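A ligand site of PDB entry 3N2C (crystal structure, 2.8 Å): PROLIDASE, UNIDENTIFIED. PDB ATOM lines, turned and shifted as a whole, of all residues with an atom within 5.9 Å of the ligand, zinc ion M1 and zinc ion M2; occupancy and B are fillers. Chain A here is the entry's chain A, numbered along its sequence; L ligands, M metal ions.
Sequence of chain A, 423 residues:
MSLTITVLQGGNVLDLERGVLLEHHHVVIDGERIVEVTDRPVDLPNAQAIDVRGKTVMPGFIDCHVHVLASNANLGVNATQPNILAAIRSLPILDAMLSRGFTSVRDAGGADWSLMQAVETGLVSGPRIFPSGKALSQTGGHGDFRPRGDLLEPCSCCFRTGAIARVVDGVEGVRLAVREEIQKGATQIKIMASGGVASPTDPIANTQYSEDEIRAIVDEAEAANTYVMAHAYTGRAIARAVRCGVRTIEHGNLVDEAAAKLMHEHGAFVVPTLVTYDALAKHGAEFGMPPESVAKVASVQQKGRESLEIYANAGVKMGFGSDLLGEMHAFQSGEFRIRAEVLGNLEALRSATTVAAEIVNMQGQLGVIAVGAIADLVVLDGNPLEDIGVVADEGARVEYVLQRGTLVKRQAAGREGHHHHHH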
ATOM      1  N   HIS A  65     -11.487  11.587   1.458  1.00  0.00           N
ATOM      2  CA  HIS A  65     -12.292  12.060   2.571  1.00  0.00           C
ATOM      3  C   HIS A  65     -11.949  13.486   2.981  1.00  0.00           C
ATOM      4  O   HIS A  65     -11.003  13.729   3.738  1.00  0.00           O
ATOM      5  CB  HIS A  65     -12.141  11.099   3.767  1.00  0.00           C
ATOM      6  CG  HIS A  65     -13.254  11.217   4.770  1.00  0.00           C
ATOM      7  ND1 HIS A  65     -14.224  10.241   4.919  1.00  0.00           N
ATOM      8  CD2 HIS A  65     -13.554  12.184   5.654  1.00  0.00           C
ATOM      9  CE1 HIS A  65     -15.068  10.612   5.874  1.00  0.00           C
ATOM     10  NE2 HIS A  65     -14.677  11.791   6.340  1.00  0.00           N
ATOM     11  N   VAL A  66     -12.717  14.442   2.474  1.00  0.00           N
ATOM     12  CA  VAL A  66     -12.568  15.842   2.873  1.00  0.00           C
ATOM     13  C   VAL A  66     -13.880  16.454   3.366  1.00  0.00           C
ATOM     14  O   VAL A  66     -14.971  15.915   3.149  1.00  0.00           O
ATOM     15  CB  VAL A  66     -11.981  16.740   1.745  1.00  0.00           C
ATOM     16  CG1 VAL A  66     -10.622  16.261   1.326  1.00  0.00           C
ATOM     17  CG2 VAL A  66     -12.909  16.797   0.553  1.00  0.00           C
ATOM     18  N   HIS A  67     -13.760  17.591   4.051  1.00  0.00           N
ATOM     19  CA  HIS A  67     -14.898  18.435   4.366  1.00  0.00           C
ATOM     20  C   HIS A  67     -14.552  19.855   3.977  1.00  0.00           C
ATOM     21  O   HIS A  67     -14.110  20.658   4.800  1.00  0.00           O
ATOM     22  CB  HIS A  67     -15.261  18.342   5.837  1.00  0.00           C
ATOM     23  CG  HIS A  67     -15.923  17.065   6.214  1.00  0.00           C
ATOM     24  ND1 HIS A  67     -17.108  16.646   5.637  1.00  0.00           N
ATOM     25  CD2 HIS A  67     -15.582  16.115   7.100  1.00  0.00           C
ATOM     26  CE1 HIS A  67     -17.458  15.478   6.152  1.00  0.00           C
ATOM     27  NE2 HIS A  67     -16.544  15.141   7.056  1.00  0.00           N
ATOM     28  N   LEU A  75     -18.093  21.726  14.256  1.00  0.00           N
ATOM     29  CA  LEU A  75     -19.074  21.401  13.221  1.00  0.00           C
ATOM     30  C   LEU A  75     -20.497  21.797  13.601  1.00  0.00           C
ATOM     31  O   LEU A  75     -21.361  21.929  12.732  1.00  0.00           O
ATOM     32  CB  LEU A  75     -19.026  19.916  12.866  1.00  0.00           C
ATOM     33  CG  LEU A  75     -17.750  19.340  12.248  1.00  0.00           C
ATOM     34  CD1 LEU A  75     -17.909  17.847  12.064  1.00  0.00           C
ATOM     35  CD2 LEU A  75     -17.413  20.006  10.923  1.00  0.00           C
ATOM     36  N   ALA A 108     -17.063  14.428   1.907  1.00  0.00           N
ATOM     37  CA  ALA A 108     -17.762  13.465   2.746  1.00  0.00           C
ATOM     38  C   ALA A 108     -18.981  14.054   3.444  1.00  0.00           C
ATOM     39  O   ALA A 108     -19.522  13.447   4.360  1.00  0.00           O
ATOM     40  CB  ALA A 108     -16.802  12.878   3.761  1.00  0.00           C
ATOM     41  N   HIS A 142     -24.405  10.991  14.608  1.00  0.00           N
ATOM     42  CA  HIS A 142     -23.146  11.711  14.448  1.00  0.00           C
ATOM     43  C   HIS A 142     -23.314  13.037  13.701  1.00  0.00           C
ATOM     44  O   HIS A 142     -22.489  13.951  13.849  1.00  0.00           O
ATOM     45  CB  HIS A 142     -22.102  10.814  13.764  1.00  0.00           C
ATOM     46  CG  HIS A 142     -20.710  11.379  13.785  1.00  0.00           C
ATOM     47  ND1 HIS A 142     -20.230  12.125  14.844  1.00  0.00           N
ATOM     48  CD2 HIS A 142     -19.700  11.313  12.890  1.00  0.00           C
ATOM     49  CE1 HIS A 142     -18.987  12.500  14.583  1.00  0.00           C
ATOM     50  NE2 HIS A 142     -18.640  12.005  13.419  1.00  0.00           N
ATOM     51  N   ILE A 164     -22.727  19.862   7.420  1.00  0.00           N
ATOM     52  CA  ILE A 164     -22.114  18.623   6.953  1.00  0.00           C
ATOM     53  C   ILE A 164     -23.161  17.541   6.664  1.00  0.00           C
ATOM     54  O   ILE A 164     -23.109  16.860   5.634  1.00  0.00           O
ATOM     55  CB  ILE A 164     -21.082  18.090   7.999  1.00  0.00           C
ATOM     56  CG1 ILE A 164     -20.050  19.174   8.358  1.00  0.00           C
ATOM     57  CG2 ILE A 164     -20.409  16.809   7.537  1.00  0.00           C
ATOM     58  CD1 ILE A 164     -19.183  19.657   7.194  1.00  0.00           C
ATOM     59  N   KCX A 190     -23.270   9.481   1.612  1.00  0.00           N
ATOM     60  CA  KCX A 190     -22.651   9.327   2.919  1.00  0.00           C
ATOM     61  CB  KCX A 190     -21.922  10.604   3.326  1.00  0.00           C
ATOM     62  CG  KCX A 190     -21.321  10.561   4.722  1.00  0.00           C
ATOM     63  CD  KCX A 190     -20.159   9.575   4.792  1.00  0.00           C
ATOM     64  CE  KCX A 190     -19.404   9.690   6.100  1.00  0.00           C
ATOM     65  NZ  KCX A 190     -18.692  11.000   6.215  1.00  0.00           N
ATOM     66  C   KCX A 190     -23.687   8.951   3.984  1.00  0.00           C
ATOM     67  O   KCX A 190     -24.792   9.500   3.999  1.00  0.00           O
ATOM     68  CX  KCX A 190     -18.078  11.326   7.339  1.00  0.00           C
ATOM     69  OQ1 KCX A 190     -18.101  10.548   8.312  1.00  0.00           O
ATOM     70  OQ2 KCX A 190     -17.479  12.406   7.439  1.00  0.00           O
ATOM     71  N   MET A 192     -23.868   7.917   8.480  1.00  0.00           N
ATOM     72  CA  MET A 192     -23.227   7.723   9.786  1.00  0.00           C
ATOM     73  C   MET A 192     -23.699   6.385  10.359  1.00  0.00           C
ATOM     74  O   MET A 192     -24.824   6.272  10.856  1.00  0.00           O
ATOM     75  CB  MET A 192     -23.580   8.866  10.743  1.00  0.00           C
ATOM     76  CG  MET A 192     -23.321  10.264  10.206  1.00  0.00           C
ATOM     77  SD  MET A 192     -21.583  10.626   9.947  1.00  0.00           S
ATOM     78  CE  MET A 192     -21.639  12.392   9.649  1.00  0.00           C
ATOM     79  N   GLY A 195     -21.240   5.819  16.135  1.00  0.00           N
ATOM     80  CA  GLY A 195     -20.900   7.012  16.885  1.00  0.00           C
ATOM     81  C   GLY A 195     -19.609   7.634  16.390  1.00  0.00           C
ATOM     82  O   GLY A 195     -18.765   6.945  15.800  1.00  0.00           O
ATOM     83  N   GLY A 196     -19.449   8.929  16.610  1.00  0.00           N
ATOM     84  CA  GLY A 196     -18.253   9.629  16.193  1.00  0.00           C
ATOM     85  C   GLY A 196     -17.671  10.493  17.295  1.00  0.00           C
ATOM     86  O   GLY A 196     -18.134  10.477  18.435  1.00  0.00           O
ATOM     87  N   VAL A 197     -16.645  11.260  16.921  1.00  0.00           N
ATOM     88  CA  VAL A 197     -15.853  12.047  17.878  1.00  0.00           C
ATOM     89  C   VAL A 197     -16.377  13.488  17.999  1.00  0.00           C
ATOM     90  O   VAL A 197     -16.407  14.048  19.095  1.00  0.00           O
ATOM     91  CB  VAL A 197     -14.357  12.053  17.482  1.00  0.00           C
ATOM     92  CG1 VAL A 197     -13.512  12.600  18.585  1.00  0.00           C
ATOM     93  CG2 VAL A 197     -13.890  10.645  17.127  1.00  0.00           C
ATOM     94  N   ALA A 198     -16.817  14.051  16.877  1.00  0.00           N
ATOM     95  CA  ALA A 198     -17.244  15.461  16.790  1.00  0.00           C
ATOM     96  C   ALA A 198     -18.581  15.762  17.472  1.00  0.00           C
ATOM     97  O   ALA A 198     -18.704  16.775  18.171  1.00  0.00           O
ATOM     98  CB  ALA A 198     -17.254  15.929  15.335  1.00  0.00           C
ATOM     99  N   SER A 199     -19.570  14.907  17.250  1.00  0.00           N
ATOM    100  CA  SER A 199     -20.907  15.059  17.846  1.00  0.00           C
ATOM    101  C   SER A 199     -20.894  14.810  19.354  1.00  0.00           C
ATOM    102  O   SER A 199     -20.253  13.855  19.815  1.00  0.00           O
ATOM    103  CB  SER A 199     -21.895  14.100  17.166  1.00  0.00           C
ATOM    104  OG  SER A 199     -21.380  12.781  17.160  1.00  0.00           O
ATOM    105  N   ILE A 204     -18.408   6.565  20.551  1.00  0.00           N
ATOM    106  CA  ILE A 204     -17.888   5.918  19.334  1.00  0.00           C
ATOM    107  C   ILE A 204     -18.128   4.403  19.289  1.00  0.00           C
ATOM    108  O   ILE A 204     -18.058   3.785  18.212  1.00  0.00           O
ATOM    109  CB  ILE A 204     -16.365   6.206  19.144  1.00  0.00           C
ATOM    110  CG1 ILE A 204     -15.555   5.727  20.353  1.00  0.00           C
ATOM    111  CG2 ILE A 204     -16.124   7.685  18.883  1.00  0.00           C
ATOM    112  CD1 ILE A 204     -14.131   5.394  20.050  1.00  0.00           C
ATOM    113  N   HIS A 231     -19.363   6.026   7.696  1.00  0.00           N
ATOM    114  CA  HIS A 231     -18.558   6.330   8.872  1.00  0.00           C
ATOM    115  C   HIS A 231     -18.802   5.282   9.969  1.00  0.00           C
ATOM    116  O   HIS A 231     -19.915   5.135  10.471  1.00  0.00           O
ATOM    117  CB  HIS A 231     -18.896   7.756   9.339  1.00  0.00           C
ATOM    118  CG  HIS A 231     -18.616   8.031  10.774  1.00  0.00           C
ATOM    119  ND1 HIS A 231     -17.403   8.523  11.209  1.00  0.00           N
ATOM    120  CD2 HIS A 231     -19.388   7.922  11.887  1.00  0.00           C
ATOM    121  CE1 HIS A 231     -17.439   8.689  12.516  1.00  0.00           C
ATOM    122  NE2 HIS A 231     -18.629   8.327  12.954  1.00  0.00           N
ATOM    123  N   TYR A 233     -16.451   3.101  13.341  1.00  0.00           N
ATOM    124  CA  TYR A 233     -15.205   2.927  14.106  1.00  0.00           C
ATOM    125  C   TYR A 233     -14.943   1.483  14.525  1.00  0.00           C
ATOM    126  O   TYR A 233     -13.919   0.906  14.156  1.00  0.00           O
ATOM    127  CB  TYR A 233     -15.186   3.839  15.330  1.00  0.00           C
ATOM    128  CG  TYR A 233     -14.790   5.255  15.007  1.00  0.00           C
ATOM    129  CD1 TYR A 233     -13.535   5.535  14.490  1.00  0.00           C
ATOM    130  CD2 TYR A 233     -15.671   6.305  15.215  1.00  0.00           C
ATOM    131  CE1 TYR A 233     -13.154   6.830  14.194  1.00  0.00           C
ATOM    132  CE2 TYR A 233     -15.300   7.620  14.915  1.00  0.00           C
ATOM    133  CZ  TYR A 233     -14.042   7.871  14.400  1.00  0.00           C
ATOM    134  OH  TYR A 233     -13.656   9.152  14.096  1.00  0.00           O
ATOM    135  N   GLU A 250     -15.228   4.626   6.259  1.00  0.00           N
ATOM    136  CA  GLU A 250     -14.384   5.747   6.676  1.00  0.00           C
ATOM    137  C   GLU A 250     -13.783   5.451   8.042  1.00  0.00           C
ATOM    138  O   GLU A 250     -14.375   4.715   8.838  1.00  0.00           O
ATOM    139  CB  GLU A 250     -15.188   7.050   6.685  1.00  0.00           C
ATOM    140  CG  GLU A 250     -16.084   7.253   5.474  1.00  0.00           C
ATOM    141  CD  GLU A 250     -15.338   7.179   4.154  1.00  0.00           C
ATOM    142  OE1 GLU A 250     -14.255   7.785   4.027  1.00  0.00           O
ATOM    143  OE2 GLU A 250     -15.842   6.510   3.226  1.00  0.00           O
ATOM    144  N   HIS A 251     -12.614   6.039   8.292  1.00  0.00           N
ATOM    145  CA  HIS A 251     -11.858   5.914   9.561  1.00  0.00           C
ATOM    146  C   HIS A 251     -11.459   4.475   9.899  1.00  0.00           C
ATOM    147  O   HIS A 251     -10.308   4.084   9.704  1.00  0.00           O
ATOM    148  CB  HIS A 251     -12.593   6.586  10.725  1.00  0.00           C
ATOM    149  CG  HIS A 251     -13.267   7.864  10.344  1.00  0.00           C
ATOM    150  ND1 HIS A 251     -12.596   9.062  10.256  1.00  0.00           N
ATOM    151  CD2 HIS A 251     -14.554   8.128  10.009  1.00  0.00           C
ATOM    152  CE1 HIS A 251     -13.444  10.010   9.878  1.00  0.00           C
ATOM    153  NE2 HIS A 251     -14.639   9.462   9.725  1.00  0.00           N
ATOM    154  N   THR A 273      -8.331   7.946   8.140  1.00  0.00           N
ATOM    155  CA  THR A 273      -7.966   9.366   8.132  1.00  0.00           C
ATOM    156  C   THR A 273      -7.195   9.680   9.402  1.00  0.00           C
ATOM    157  O   THR A 273      -7.729  10.255  10.340  1.00  0.00           O
ATOM    158  CB  THR A 273      -9.219  10.281   8.045  1.00  0.00           C
ATOM    159  OG1 THR A 273     -10.093  10.008   9.148  1.00  0.00           O
ATOM    160  CG2 THR A 273      -9.988  10.073   6.752  1.00  0.00           C
ATOM    161  N   THR A 276      -6.011  13.565  11.152  1.00  0.00           N
ATOM    162  CA  THR A 276      -6.941  14.451  11.865  1.00  0.00           C
ATOM    163  C   THR A 276      -6.871  14.296  13.387  1.00  0.00           C
ATOM    164  O   THR A 276      -7.016  15.280  14.110  1.00  0.00           O
ATOM    165  CB  THR A 276      -8.394  14.369  11.307  1.00  0.00           C
ATOM    166  OG1 THR A 276      -9.226  15.323  11.987  1.00  0.00           O
ATOM    167  CG2 THR A 276      -8.996  12.984  11.450  1.00  0.00           C
ATOM    168  N   TYR A 277      -6.619  13.069  13.854  1.00  0.00           N
ATOM    169  CA  TYR A 277      -6.554  12.785  15.277  1.00  0.00           C
ATOM    170  C   TYR A 277      -5.261  13.307  15.890  1.00  0.00           C
ATOM    171  O   TYR A 277      -5.250  13.762  17.038  1.00  0.00           O
ATOM    172  CB  TYR A 277      -6.696  11.282  15.516  1.00  0.00           C
ATOM    173  CG  TYR A 277      -7.895  10.675  14.847  1.00  0.00           C
ATOM    174  CD1 TYR A 277      -9.190  10.937  15.308  1.00  0.00           C
ATOM    175  CD2 TYR A 277      -7.743   9.851  13.732  1.00  0.00           C
ATOM    176  CE1 TYR A 277     -10.300  10.395  14.678  1.00  0.00           C
ATOM    177  CE2 TYR A 277      -8.851   9.295  13.103  1.00  0.00           C
ATOM    178  CZ  TYR A 277     -10.132   9.567  13.580  1.00  0.00           C
ATOM    179  OH  TYR A 277     -11.222   9.021  12.959  1.00  0.00           O
ATOM    180  N   LEU A 280      -5.852  16.988  16.162  1.00  0.00           N
ATOM    181  CA  LEU A 280      -6.744  17.237  17.306  1.00  0.00           C
ATOM    182  C   LEU A 280      -6.122  16.822  18.650  1.00  0.00           C
ATOM    183  O   LEU A 280      -6.689  17.086  19.707  1.00  0.00           O
ATOM    184  CB  LEU A 280      -8.098  16.550  17.105  1.00  0.00           C
ATOM    185  CG  LEU A 280      -9.008  17.073  15.982  1.00  0.00           C
ATOM    186  CD1 LEU A 280     -10.189  16.136  15.763  1.00  0.00           C
ATOM    187  CD2 LEU A 280      -9.467  18.503  16.242  1.00  0.00           C
ATOM    188  N   ASP A 323      -9.670  14.299   6.361  1.00  0.00           N
ATOM    189  CA  ASP A 323     -10.777  14.633   7.287  1.00  0.00           C
ATOM    190  C   ASP A 323     -10.444  15.796   8.242  1.00  0.00           C
ATOM    191  O   ASP A 323     -10.860  15.817   9.403  1.00  0.00           O
ATOM    192  CB  ASP A 323     -11.227  13.376   8.044  1.00  0.00           C
ATOM    193  CG  ASP A 323     -12.585  13.523   8.707  1.00  0.00           C
ATOM    194  OD1 ASP A 323     -13.516  14.069   8.067  1.00  0.00           O
ATOM    195  OD2 ASP A 323     -12.723  13.093   9.866  1.00  0.00           O
ATOM    196  N   LEU A 325     -10.423  19.713   9.693  1.00  0.00           N
ATOM    197  CA  LEU A 325     -11.429  20.764   9.845  1.00  0.00           C
ATOM    198  C   LEU A 325     -10.768  22.109  10.134  1.00  0.00           C
ATOM    199  O   LEU A 325      -9.811  22.190  10.910  1.00  0.00           O
ATOM    200  CB  LEU A 325     -12.406  20.415  10.980  1.00  0.00           C
ATOM    201  CG  LEU A 325     -12.896  18.982  11.151  1.00  0.00           C
ATOM    202  CD1 LEU A 325     -13.459  18.785  12.545  1.00  0.00           C
ATOM    203  CD2 LEU A 325     -13.918  18.565  10.099  1.00  0.00           C
HETATM  204  C1  LIG L   1     -15.365  11.979  13.892  1.00  0.00           C
HETATM  205  N1  LIG L   1     -14.787  13.573  12.105  1.00  0.00           N
HETATM  206  O1  LIG L   1     -15.614  10.783  14.135  1.00  0.00           O
HETATM  207  P1  LIG L   1     -16.064  13.671  11.032  1.00  0.00           P
HETATM  208  C2  LIG L   1     -16.110  15.254  10.357  1.00  0.00           C
HETATM  209  O2  LIG L   1     -17.420  13.493  11.864  1.00  0.00           O
HETATM  210  O3  LIG L   1     -15.797  12.711   9.903  1.00  0.00           O
HETATM  211  C3  LIG L   1     -14.427  12.316  12.762  1.00  0.00           C
HETATM  212  C4  LIG L   1     -13.024  12.575  13.296  1.00  0.00           C
HETATM  213  C5  LIG L   1     -13.938  14.705  12.469  1.00  0.00           C
HETATM  214  C6  LIG L   1     -12.733  14.053  13.134  1.00  0.00           C
HETATM  215  O4  LIG L   1     -15.875  12.908  14.540  1.00  0.00           O
HETATM  216 ZN    ZN M   1     -15.700  13.183   7.620  1.00  0.00          ZN
HETATM  217 ZN    ZN M   2     -16.988  10.665  10.098  1.00  0.00          ZN
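Of the 25 residues printed, 4 come within 4 Å of zinc ion M1.
Residues that only touch the ligand: Leu 75, Gly 196, Thr 276, Tyr 277 and Leu 325.
Hydrophobic or aromatic side chains within 4 Å of the ligand: His 67, Leu 75, His 142, Val 197, Ala 198, His 231, Tyr 233, His 251, Tyr 277 and Leu 325.
15 residues have an atom within 4 Å of the ligand: His 65, His 67, Leu 75, His 142, KCX 190, Gly 196, Val 197, Ala 198, His 231, Tyr 233, His 251, Thr 276, Tyr 277, Asp 323 and Leu 325.
The nearest printed residue that does not touch the ligand is Leu 280 (4.2 Å).
NZ of KCX 190 sits at hydrogen-bond distance from the backbone carbonyl oxygen of Ala 108, 3.2 Å away.
The side-chain carboxylate of Glu 250 lies within hydrogen-bond range of a ring nitrogen (ND1) of His 65 (2.6 Å).
O of Asp 323 is in hydrogen-bond range of OG1 of Thr 276.
NE2 of His 231 sits at hydrogen-bond distance from O of Gly 195 (3.2 Å).
A ring nitrogen (ND1) of His 142 sits at hydrogen-bond distance from the side-chain hydroxyl of Ser 199.
The side-chain hydroxyl (OH) of Tyr 277 lies within hydrogen-bond range of the side-chain hydroxyl (OH) of Tyr 233, 2.7 Å away.
ND1 of His 251 lies within hydrogen-bond range of OH of Tyr 277 (3.0 Å).
A ring nitrogen (ND1) of His 251 is in hydrogen-bond range of the side-chain hydroxyl (OG1) of Thr 273 (2.9 Å).
Zinc ion M2 is bound by OQ1 of KCX 190 (2.1 Å), O3 of the ligand (2.4 Å), ND1 of His 231 (2.4 Å) and NE2 of His 251 (2.7 Å).
NE2 of His 142 lies within hydrogen-bond range of O2 of the ligand, 2.5 Å away.
The side-chain hydroxyl of Tyr 233 is in hydrogen-bond range of an oxygen (O1) of the ligand (2.5 Å).
N of Ala 198 lies within hydrogen-bond range of O4 of the ligand (2.8 Å).
The backbone NH (N) of Val 197 sits at hydrogen-bond distance from an oxygen (O4) of the ligand, at 3.0 Å.
Zinc ion M1 is bound by OQ2 of KCX 190 (1.9 Å), NE2 of His 65 (2.2 Å), NE2 of His 67 (2.2 Å), O3 of the ligand (2.3 Å) and OD1 of Asp 323 (2.4 Å).
Zinc ion M1 has five donor atoms within binding distance.
Merely in contact with zinc ion M2: His 142.
Four residues have an atom within 4 Å of zinc ion M2: His 142, KCX 190, His 231 and His 251.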
